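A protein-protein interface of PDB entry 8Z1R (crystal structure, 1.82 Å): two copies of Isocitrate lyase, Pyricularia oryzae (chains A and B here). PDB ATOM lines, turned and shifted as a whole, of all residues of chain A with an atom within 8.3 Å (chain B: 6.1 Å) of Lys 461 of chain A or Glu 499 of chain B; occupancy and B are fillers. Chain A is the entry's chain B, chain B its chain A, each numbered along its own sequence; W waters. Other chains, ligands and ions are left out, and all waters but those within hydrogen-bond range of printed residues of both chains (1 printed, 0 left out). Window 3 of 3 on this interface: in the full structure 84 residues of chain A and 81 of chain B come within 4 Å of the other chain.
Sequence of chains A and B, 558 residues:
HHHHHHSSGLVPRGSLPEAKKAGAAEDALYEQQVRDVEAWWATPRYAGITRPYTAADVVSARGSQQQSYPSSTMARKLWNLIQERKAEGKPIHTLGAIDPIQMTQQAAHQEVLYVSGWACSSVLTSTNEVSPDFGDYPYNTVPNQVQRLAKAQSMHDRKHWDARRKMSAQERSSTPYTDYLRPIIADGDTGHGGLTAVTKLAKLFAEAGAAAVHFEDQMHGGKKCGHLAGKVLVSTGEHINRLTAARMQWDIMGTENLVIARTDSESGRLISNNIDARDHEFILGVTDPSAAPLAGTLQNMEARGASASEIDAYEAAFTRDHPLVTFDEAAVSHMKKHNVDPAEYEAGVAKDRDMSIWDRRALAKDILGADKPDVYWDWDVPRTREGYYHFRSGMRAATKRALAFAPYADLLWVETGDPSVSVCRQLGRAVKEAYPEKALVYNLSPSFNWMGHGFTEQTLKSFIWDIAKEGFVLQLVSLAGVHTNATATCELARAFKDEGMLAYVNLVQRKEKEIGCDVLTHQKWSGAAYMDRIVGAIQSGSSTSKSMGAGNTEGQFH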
ATOM      1  N   HIS A  93     -33.846 -29.165 -17.962  1.00  0.00           N
ATOM      2  CA  HIS A  93     -33.816 -28.959 -16.519  1.00  0.00           C
ATOM      3  C   HIS A  93     -35.240 -28.872 -15.993  1.00  0.00           C
ATOM      4  O   HIS A  93     -36.084 -28.195 -16.587  1.00  0.00           O
ATOM      5  CB  HIS A  93     -33.023 -27.702 -16.138  1.00  0.00           C
ATOM      6  CG  HIS A  93     -33.388 -26.465 -16.912  1.00  0.00           C
ATOM      7  ND1 HIS A  93     -33.485 -26.437 -18.288  1.00  0.00           N
ATOM      8  CD2 HIS A  93     -33.600 -25.193 -16.496  1.00  0.00           C
ATOM      9  CE1 HIS A  93     -33.779 -25.207 -18.679  1.00  0.00           C
ATOM     10  NE2 HIS A  93     -33.843 -24.429 -17.613  1.00  0.00           N
ATOM     11  N   TRP A 450     -24.818 -22.654  -2.504  1.00  0.00           N
ATOM     12  CA  TRP A 450     -24.070 -22.279  -3.702  1.00  0.00           C
ATOM     13  C   TRP A 450     -23.263 -21.001  -3.490  1.00  0.00           C
ATOM     14  O   TRP A 450     -22.046 -20.979  -3.698  1.00  0.00           O
ATOM     15  CB  TRP A 450     -25.028 -22.095  -4.890  1.00  0.00           C
ATOM     16  CG  TRP A 450     -25.848 -23.295  -5.256  1.00  0.00           C
ATOM     17  CD1 TRP A 450     -26.966 -23.770  -4.607  1.00  0.00           C
ATOM     18  CD2 TRP A 450     -25.641 -24.164  -6.377  1.00  0.00           C
ATOM     19  NE1 TRP A 450     -27.448 -24.884  -5.252  1.00  0.00           N
ATOM     20  CE2 TRP A 450     -26.654 -25.150  -6.340  1.00  0.00           C
ATOM     21  CE3 TRP A 450     -24.686 -24.216  -7.398  1.00  0.00           C
ATOM     22  CZ2 TRP A 450     -26.745 -26.164  -7.294  1.00  0.00           C
ATOM     23  CZ3 TRP A 450     -24.792 -25.211  -8.354  1.00  0.00           C
ATOM     24  CH2 TRP A 450     -25.800 -26.181  -8.287  1.00  0.00           C
ATOM     25  N   MET A 451     -23.930 -19.926  -3.065  1.00  0.00           N
ATOM     26  CA  MET A 451     -23.284 -18.622  -2.955  1.00  0.00           C
ATOM     27  C   MET A 451     -22.292 -18.541  -1.804  1.00  0.00           C
ATOM     28  O   MET A 451     -21.481 -17.613  -1.774  1.00  0.00           O
ATOM     29  CB  MET A 451     -24.334 -17.520  -2.795  1.00  0.00           C
ATOM     30  CG  MET A 451     -25.261 -17.381  -3.992  1.00  0.00           C
ATOM     31  SD  MET A 451     -24.391 -16.919  -5.512  1.00  0.00           S
ATOM     32  CE  MET A 451     -23.608 -15.353  -5.053  1.00  0.00           C
ATOM     33  N   PHE A 455     -19.575 -19.878  -5.716  1.00  0.00           N
ATOM     34  CA  PHE A 455     -20.302 -19.437  -6.899  1.00  0.00           C
ATOM     35  C   PHE A 455     -20.516 -17.928  -6.846  1.00  0.00           C
ATOM     36  O   PHE A 455     -20.603 -17.340  -5.768  1.00  0.00           O
ATOM     37  CB  PHE A 455     -21.640 -20.177  -7.023  1.00  0.00           C
ATOM     38  CG  PHE A 455     -21.490 -21.571  -7.558  1.00  0.00           C
ATOM     39  CD1 PHE A 455     -21.059 -22.603  -6.726  1.00  0.00           C
ATOM     40  CD2 PHE A 455     -21.707 -21.840  -8.899  1.00  0.00           C
ATOM     41  CE1 PHE A 455     -20.879 -23.883  -7.219  1.00  0.00           C
ATOM     42  CE2 PHE A 455     -21.528 -23.127  -9.404  1.00  0.00           C
ATOM     43  CZ  PHE A 455     -21.112 -24.145  -8.569  1.00  0.00           C
ATOM     44  N   THR A 456     -20.546 -17.299  -8.020  1.00  0.00           N
ATOM     45  CA  THR A 456     -21.054 -15.946  -8.162  1.00  0.00           C
ATOM     46  C   THR A 456     -22.483 -16.029  -8.671  1.00  0.00           C
ATOM     47  O   THR A 456     -22.963 -17.090  -9.089  1.00  0.00           O
ATOM     48  CB  THR A 456     -20.202 -15.114  -9.132  1.00  0.00           C
ATOM     49  OG1 THR A 456     -20.373 -15.628 -10.456  1.00  0.00           O
ATOM     50  CG2 THR A 456     -18.716 -15.162  -8.760  1.00  0.00           C
ATOM     51  N   GLU A 457     -23.172 -14.891  -8.646  1.00  0.00           N
ATOM     52  CA  GLU A 457     -24.530 -14.901  -9.172  1.00  0.00           C
ATOM     53  C   GLU A 457     -24.533 -15.329 -10.629  1.00  0.00           C
ATOM     54  O   GLU A 457     -25.418 -16.073 -11.063  1.00  0.00           O
ATOM     55  CB  GLU A 457     -25.180 -13.535  -8.997  1.00  0.00           C
ATOM     56  CG  GLU A 457     -25.548 -13.253  -7.555  1.00  0.00           C
ATOM     57  CD  GLU A 457     -26.757 -12.352  -7.446  1.00  0.00           C
ATOM     58  OE1 GLU A 457     -27.228 -11.870  -8.501  1.00  0.00           O
ATOM     59  OE2 GLU A 457     -27.238 -12.139  -6.313  1.00  0.00           O
ATOM     60  N   GLN A 458     -23.513 -14.912 -11.382  1.00  0.00           N
ATOM     61  CA  GLN A 458     -23.427 -15.257 -12.798  1.00  0.00           C
ATOM     62  C   GLN A 458     -23.128 -16.743 -13.017  1.00  0.00           C
ATOM     63  O   GLN A 458     -23.720 -17.373 -13.901  1.00  0.00           O
ATOM     64  CB  GLN A 458     -22.367 -14.384 -13.470  1.00  0.00           C
ATOM     65  CG  GLN A 458     -21.936 -14.853 -14.850  1.00  0.00           C
ATOM     66  CD  GLN A 458     -20.516 -14.426 -15.196  1.00  0.00           C
ATOM     67  OE1 GLN A 458     -19.574 -15.220 -15.097  1.00  0.00           O
ATOM     68  NE2 GLN A 458     -20.358 -13.168 -15.607  1.00  0.00           N
ATOM     69  N   THR A 459     -22.190 -17.323 -12.261  1.00  0.00           N
ATOM     70  CA  THR A 459     -21.914 -18.739 -12.480  1.00  0.00           C
ATOM     71  C   THR A 459     -22.954 -19.640 -11.827  1.00  0.00           C
ATOM     72  O   THR A 459     -23.077 -20.801 -12.223  1.00  0.00           O
ATOM     73  CB  THR A 459     -20.518 -19.138 -11.986  1.00  0.00           C
ATOM     74  OG1 THR A 459     -20.444 -19.016 -10.561  1.00  0.00           O
ATOM     75  CG2 THR A 459     -19.441 -18.267 -12.646  1.00  0.00           C
ATOM     76  N   LEU A 460     -23.683 -19.142 -10.829  1.00  0.00           N
ATOM     77  CA  LEU A 460     -24.837 -19.871 -10.323  1.00  0.00           C
ATOM     78  C   LEU A 460     -25.888 -20.001 -11.417  1.00  0.00           C
ATOM     79  O   LEU A 460     -26.411 -21.093 -11.677  1.00  0.00           O
ATOM     80  CB  LEU A 460     -25.411 -19.154  -9.099  1.00  0.00           C
ATOM     81  CG  LEU A 460     -26.696 -19.763  -8.512  1.00  0.00           C
ATOM     82  CD1 LEU A 460     -26.463 -21.215  -8.119  1.00  0.00           C
ATOM     83  CD2 LEU A 460     -27.156 -18.942  -7.293  1.00  0.00           C
ATOM     84  N   LYS A 461     -26.157 -18.895 -12.113  1.00  0.00           N
ATOM     85  CA  LYS A 461     -27.117 -18.924 -13.210  1.00  0.00           C
ATOM     86  C   LYS A 461     -26.635 -19.815 -14.346  1.00  0.00           C
ATOM     87  O   LYS A 461     -27.425 -20.577 -14.912  1.00  0.00           O
ATOM     88  CB  LYS A 461     -27.384 -17.504 -13.711  1.00  0.00           C
ATOM     89  CG  LYS A 461     -28.155 -17.451 -15.009  1.00  0.00           C
ATOM     90  CD  LYS A 461     -28.621 -16.035 -15.333  1.00  0.00           C
ATOM     91  CE  LYS A 461     -29.144 -15.980 -16.766  1.00  0.00           C
ATOM     92  NZ  LYS A 461     -29.613 -14.612 -17.135  1.00  0.00           N
ATOM     93  N   SER A 462     -25.344 -19.762 -14.684  1.00  0.00           N
ATOM     94  CA  SER A 462     -24.918 -20.478 -15.880  1.00  0.00           C
ATOM     95  C   SER A 462     -24.667 -21.959 -15.635  1.00  0.00           C
ATOM     96  O   SER A 462     -24.541 -22.700 -16.613  1.00  0.00           O
ATOM     97  CB  SER A 462     -23.664 -19.823 -16.493  1.00  0.00           C
ATOM     98  OG  SER A 462     -22.531 -19.913 -15.643  1.00  0.00           O
ATOM     99  N   PHE A 463     -24.645 -22.409 -14.371  1.00  0.00           N
ATOM    100  CA  PHE A 463     -24.229 -23.775 -14.044  1.00  0.00           C
ATOM    101  C   PHE A 463     -24.964 -24.824 -14.881  1.00  0.00           C
ATOM    102  O   PHE A 463     -24.342 -25.720 -15.461  1.00  0.00           O
ATOM    103  CB  PHE A 463     -24.440 -24.049 -12.550  1.00  0.00           C
ATOM    104  CG  PHE A 463     -24.012 -25.421 -12.133  1.00  0.00           C
ATOM    105  CD1 PHE A 463     -22.676 -25.701 -11.922  1.00  0.00           C
ATOM    106  CD2 PHE A 463     -24.939 -26.446 -11.990  1.00  0.00           C
ATOM    107  CE1 PHE A 463     -22.273 -26.963 -11.545  1.00  0.00           C
ATOM    108  CE2 PHE A 463     -24.541 -27.716 -11.628  1.00  0.00           C
ATOM    109  CZ  PHE A 463     -23.206 -27.972 -11.398  1.00  0.00           C
ATOM    110  N   ILE A 464     -26.298 -24.736 -14.934  1.00  0.00           N
ATOM    111  CA  ILE A 464     -27.089 -25.713 -15.681  1.00  0.00           C
ATOM    112  C   ILE A 464     -26.651 -25.752 -17.144  1.00  0.00           C
ATOM    113  O   ILE A 464     -26.462 -26.832 -17.729  1.00  0.00           O
ATOM    114  CB  ILE A 464     -28.587 -25.382 -15.529  1.00  0.00           C
ATOM    115  CG1 ILE A 464     -29.049 -25.719 -14.099  1.00  0.00           C
ATOM    116  CG2 ILE A 464     -29.415 -26.064 -16.619  1.00  0.00           C
ATOM    117  CD1 ILE A 464     -30.496 -25.316 -13.800  1.00  0.00           C
ATOM    118  N   TRP A 465     -26.449 -24.581 -17.747  1.00  0.00           N
ATOM    119  CA  TRP A 465     -26.032 -24.542 -19.148  1.00  0.00           C
ATOM    120  C   TRP A 465     -24.574 -24.948 -19.318  1.00  0.00           C
ATOM    121  O   TRP A 465     -24.230 -25.597 -20.318  1.00  0.00           O
ATOM    122  CB  TRP A 465     -26.310 -23.144 -19.723  1.00  0.00           C
ATOM    123  CG  TRP A 465     -27.803 -22.953 -19.886  1.00  0.00           C
ATOM    124  CD1 TRP A 465     -28.544 -23.266 -20.984  1.00  0.00           C
ATOM    125  CD2 TRP A 465     -28.727 -22.460 -18.901  1.00  0.00           C
ATOM    126  NE1 TRP A 465     -29.874 -22.979 -20.758  1.00  0.00           N
ATOM    127  CE2 TRP A 465     -30.014 -22.491 -19.485  1.00  0.00           C
ATOM    128  CE3 TRP A 465     -28.586 -21.986 -17.588  1.00  0.00           C
ATOM    129  CZ2 TRP A 465     -31.167 -22.087 -18.796  1.00  0.00           C
ATOM    130  CZ3 TRP A 465     -29.714 -21.584 -16.900  1.00  0.00           C
ATOM    131  CH2 TRP A 465     -31.000 -21.617 -17.517  1.00  0.00           C
ATOM    132  N   ASP A 466     -23.721 -24.629 -18.336  1.00  0.00           N
ATOM    133  CA  ASP A 466     -22.318 -25.041 -18.401  1.00  0.00           C
ATOM    134  C   ASP A 466     -22.167 -26.563 -18.433  1.00  0.00           C
ATOM    135  O   ASP A 466     -21.336 -27.102 -19.180  1.00  0.00           O
ATOM    136  CB  ASP A 466     -21.537 -24.493 -17.203  1.00  0.00           C
ATOM    137  CG  ASP A 466     -21.436 -22.977 -17.196  1.00  0.00           C
ATOM    138  OD1 ASP A 466     -21.496 -22.355 -18.289  1.00  0.00           O
ATOM    139  OD2 ASP A 466     -21.302 -22.413 -16.080  1.00  0.00           O
ATOM    140  N   ARG B 494     -41.602 -20.349 -14.277  1.00  0.00           N
ATOM    141  CA  ARG B 494     -41.241 -19.340 -15.277  1.00  0.00           C
ATOM    142  C   ARG B 494     -39.783 -18.918 -15.156  1.00  0.00           C
ATOM    143  O   ARG B 494     -39.072 -18.782 -16.163  1.00  0.00           O
ATOM    144  CB  ARG B 494     -42.120 -18.095 -15.118  1.00  0.00           C
ATOM    145  CG  ARG B 494     -43.569 -18.271 -15.411  1.00  0.00           C
ATOM    146  CD  ARG B 494     -44.169 -16.905 -15.702  1.00  0.00           C
ATOM    147  NE  ARG B 494     -45.607 -16.994 -15.886  1.00  0.00           N
ATOM    148  CZ  ARG B 494     -46.484 -16.241 -15.244  1.00  0.00           C
ATOM    149  NH1 ARG B 494     -46.095 -15.295 -14.400  1.00  0.00           N
ATOM    150  NH2 ARG B 494     -47.784 -16.429 -15.463  1.00  0.00           N
ATOM    151  N   ALA B 495     -39.334 -18.655 -13.929  1.00  0.00           N
ATOM    152  CA  ALA B 495     -38.001 -18.092 -13.723  1.00  0.00           C
ATOM    153  C   ALA B 495     -36.908 -19.141 -13.903  1.00  0.00           C
ATOM    154  O   ALA B 495     -35.822 -18.838 -14.413  1.00  0.00           O
ATOM    155  CB  ALA B 495     -37.914 -17.472 -12.332  1.00  0.00           C
ATOM    156  N   PHE B 496     -37.176 -20.376 -13.478  1.00  0.00           N
ATOM    157  CA  PHE B 496     -36.188 -21.453 -13.564  1.00  0.00           C
ATOM    158  C   PHE B 496     -35.833 -21.772 -15.011  1.00  0.00           C
ATOM    159  O   PHE B 496     -34.697 -22.156 -15.307  1.00  0.00           O
ATOM    160  CB  PHE B 496     -36.758 -22.689 -12.853  1.00  0.00           C
ATOM    161  CG  PHE B 496     -35.832 -23.851 -12.794  1.00  0.00           C
ATOM    162  CD1 PHE B 496     -34.743 -23.838 -11.938  1.00  0.00           C
ATOM    163  CD2 PHE B 496     -36.076 -24.982 -13.562  1.00  0.00           C
ATOM    164  CE1 PHE B 496     -33.898 -24.923 -11.855  1.00  0.00           C
ATOM    165  CE2 PHE B 496     -35.228 -26.075 -13.486  1.00  0.00           C
ATOM    166  CZ  PHE B 496     -34.130 -26.031 -12.644  1.00  0.00           C
ATOM    167  N   LYS B 497     -36.793 -21.621 -15.926  1.00  0.00           N
ATOM    168  CA  LYS B 497     -36.522 -21.898 -17.332  1.00  0.00           C
ATOM    169  C   LYS B 497     -35.350 -21.071 -17.856  1.00  0.00           C
ATOM    170  O   LYS B 497     -34.522 -21.580 -18.619  1.00  0.00           O
ATOM    171  CB  LYS B 497     -37.777 -21.625 -18.161  1.00  0.00           C
ATOM    172  CG  LYS B 497     -37.621 -21.886 -19.651  1.00  0.00           C
ATOM    173  CD  LYS B 497     -38.899 -21.475 -20.411  1.00  0.00           C
ATOM    174  CE  LYS B 497     -38.719 -21.589 -21.927  1.00  0.00           C
ATOM    175  NZ  LYS B 497     -40.039 -21.598 -22.645  1.00  0.00           N
ATOM    176  N   ASP B 498     -35.275 -19.790 -17.476  1.00  0.00           N
ATOM    177  CA  ASP B 498     -34.250 -18.891 -18.010  1.00  0.00           C
ATOM    178  C   ASP B 498     -33.094 -18.617 -17.056  1.00  0.00           C
ATOM    179  O   ASP B 498     -31.988 -18.302 -17.520  1.00  0.00           O
ATOM    180  CB  ASP B 498     -34.866 -17.546 -18.397  1.00  0.00           C
ATOM    181  CG  ASP B 498     -35.950 -17.680 -19.443  1.00  0.00           C
ATOM    182  OD1 ASP B 498     -35.717 -18.344 -20.479  1.00  0.00           O
ATOM    183  OD2 ASP B 498     -37.036 -17.110 -19.222  1.00  0.00           O
ATOM    184  N   GLU B 499     -33.318 -18.712 -15.744  1.00  0.00           N
ATOM    185  CA  GLU B 499     -32.312 -18.347 -14.756  1.00  0.00           C
ATOM    186  C   GLU B 499     -31.779 -19.531 -13.969  1.00  0.00           C
ATOM    187  O   GLU B 499     -30.834 -19.358 -13.184  1.00  0.00           O
ATOM    188  CB  GLU B 499     -32.875 -17.298 -13.780  1.00  0.00           C
ATOM    189  CG  GLU B 499     -33.390 -16.034 -14.485  1.00  0.00           C
ATOM    190  CD  GLU B 499     -32.288 -15.030 -14.779  1.00  0.00           C
ATOM    191  OE1 GLU B 499     -31.750 -14.430 -13.819  1.00  0.00           O
ATOM    192  OE2 GLU B 499     -31.951 -14.842 -15.969  1.00  0.00           O
ATOM    193  N   GLY B 500     -32.355 -20.719 -14.141  1.00  0.00           N
ATOM    194  CA  GLY B 500     -31.766 -21.903 -13.546  1.00  0.00           C
ATOM    195  C   GLY B 500     -31.657 -21.813 -12.037  1.00  0.00           C
ATOM    196  O   GLY B 500     -32.570 -21.368 -11.341  1.00  0.00           O
ATOM    197  N   MET B 501     -30.513 -22.258 -11.512  1.00  0.00           N
ATOM    198  CA  MET B 501     -30.353 -22.299 -10.063  1.00  0.00           C
ATOM    199  C   MET B 501     -30.330 -20.912  -9.429  1.00  0.00           C
ATOM    200  O   MET B 501     -30.545 -20.806  -8.220  1.00  0.00           O
ATOM    201  CB  MET B 501     -29.083 -23.075  -9.683  1.00  0.00           C
ATOM    202  CG  MET B 501     -29.168 -24.567  -9.983  1.00  0.00           C
ATOM    203  SD  MET B 501     -30.659 -25.394  -9.345  1.00  0.00           S
ATOM    204  CE  MET B 501     -30.497 -25.240  -7.573  1.00  0.00           C
ATOM    205  N   LEU B 502     -30.065 -19.849 -10.197  1.00  0.00           N
ATOM    206  CA  LEU B 502     -30.172 -18.507  -9.623  1.00  0.00           C
ATOM    207  C   LEU B 502     -31.606 -18.213  -9.212  1.00  0.00           C
ATOM    208  O   LEU B 502     -31.853 -17.662  -8.130  1.00  0.00           O
ATOM    209  CB  LEU B 502     -29.677 -17.456 -10.622  1.00  0.00           C
ATOM    210  CG  LEU B 502     -29.758 -15.990 -10.156  1.00  0.00           C
ATOM    211  CD1 LEU B 502     -29.040 -15.802  -8.821  1.00  0.00           C
ATOM    212  CD2 LEU B 502     -29.166 -15.060 -11.202  1.00  0.00           C
ATOM    213  N   ALA B 503     -32.568 -18.601 -10.055  1.00  0.00           N
ATOM    214  CA  ALA B 503     -33.971 -18.445  -9.688  1.00  0.00           C
ATOM    215  C   ALA B 503     -34.324 -19.314  -8.490  1.00  0.00           C
ATOM    216  O   ALA B 503     -35.046 -18.861  -7.594  1.00  0.00           O
ATOM    217  CB  ALA B 503     -34.878 -18.776 -10.873  1.00  0.00           C
ATOM    218  N   TYR B 504     -33.836 -20.563  -8.449  1.00  0.00           N
ATOM    219  CA  TYR B 504     -34.168 -21.411  -7.303  1.00  0.00           C
ATOM    220  C   TYR B 504     -33.645 -20.799  -6.003  1.00  0.00           C
ATOM    221  O   TYR B 504     -34.368 -20.733  -5.001  1.00  0.00           O
ATOM    222  CB  TYR B 504     -33.640 -22.845  -7.470  1.00  0.00           C
ATOM    223  CG  TYR B 504     -34.141 -23.691  -6.318  1.00  0.00           C
ATOM    224  CD1 TYR B 504     -35.403 -24.275  -6.357  1.00  0.00           C
ATOM    225  CD2 TYR B 504     -33.400 -23.812  -5.147  1.00  0.00           C
ATOM    226  CE1 TYR B 504     -35.882 -25.002  -5.283  1.00  0.00           C
ATOM    227  CE2 TYR B 504     -33.884 -24.534  -4.063  1.00  0.00           C
ATOM    228  CZ  TYR B 504     -35.127 -25.117  -4.144  1.00  0.00           C
ATOM    229  OH  TYR B 504     -35.616 -25.821  -3.070  1.00  0.00           O
HETATM  230  O   HOH W   1     -28.117 -22.539 -13.206  1.00  0.00           O
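No position is printed for both chains.
Of the 15 pairs that touch across the chains among the printed residues, none has its exchanged pair printed and touching as well.
Printed residues of chain B within 4 Å of Lys 461 of chain A: Asp 498, Glu 499 and Leu 502.
Glu 499 of chain B touches just one residue of chain A: Lys 461.
Printed residues of chain B within 4 Å of His 93 of chain A: Phe 496 and Lys 497.
Of the printed residues of chain A, Phe 496 of chain B touches His 93 (3.3 Å) and Ile 464 (3.9 Å).
Ser 462 of chain A touches none of the printed residues of chain B.
Thr 456 of chain A touches none of the printed residues of chain B.
The nearest residue of chain B that does not touch Lys 461 of chain A is Gly 500 of chain B (4.7 Å).
N of Phe 455 of chain A is in hydrogen-bond range of O of Trp 450 of chain A (3.4 Å).
Water W1 lies within hydrogen-bond range of O of Lys 461 of chain A (2.7 Å), O of Leu 460 of chain A (2.7 Å), N of Met 501 of chain B (2.9 Å) and N of Ile 464 of chain A (3.3 Å).
A ring nitrogen (NE2) of His 93 of chain A lies within hydrogen-bond range of the backbone carbonyl oxygen (O) of Phe 496 of chain B, at 3.3 Å.
The backbone carbonyl oxygen (O) of Lys 497 of chain B is in hydrogen-bond range of a ring nitrogen (NE2) of His 93 of chain A, 3.1 Å away.
The side-chain carboxylate (OE2) of Glu 499 of chain B lies within salt-bridge range of the side-chain amino group (NZ) of Lys 461 of chain A, 2.6 Å away.
Printed residues of chain A that touch a printed residue of chain B: His 93, Trp 450, Glu 457, Leu 460, Lys 461, Ile 464 and Trp 465.
Hydrophobic or aromatic side chains of chain A that line the printed part of chain B: His 93, Trp 450, Leu 460, Ile 464 and Trp 465.
Along chain A the printed residues that touch a printed residue of chain B span positions 93 to 465.
Of the 11 printed residues of chain B, 7 touch a printed residue of chain A.
Along chain B the printed residues that touch a printed residue of chain A span positions 496 to 502.
Among the printed residues, Asp or Glu carboxylates within 4 Å of a Lys or Arg side-chain nitrogen of the other chain: Lys 461 of chain A with Glu 499 of chain B (2.6 Å).
Among the printed residues, merely in contact across the chains: Trp 450 of chain A with Met 501 of chain B, Glu 457 of chain A with Leu 502 of chain B, Leu 460 of chain A with Met 501 of chain B, Leu 460 of chain A with Leu 502 of chain B, Lys 461 of chain A with Asp 498 of chain B, Lys 461 of chain A with Leu 502 of chain B, Ile 464 of chain A with Phe 496 of chain B, Ile 464 of chain A with Gly 500 of chain B, Ile 464 of chain A with Met 501 of chain B, Trp 465 of chain A with Lys 497 of chain B, Trp 465 of chain A with Asp 498 of chain B and Trp 465 of chain A with Gly 500 of chain B.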
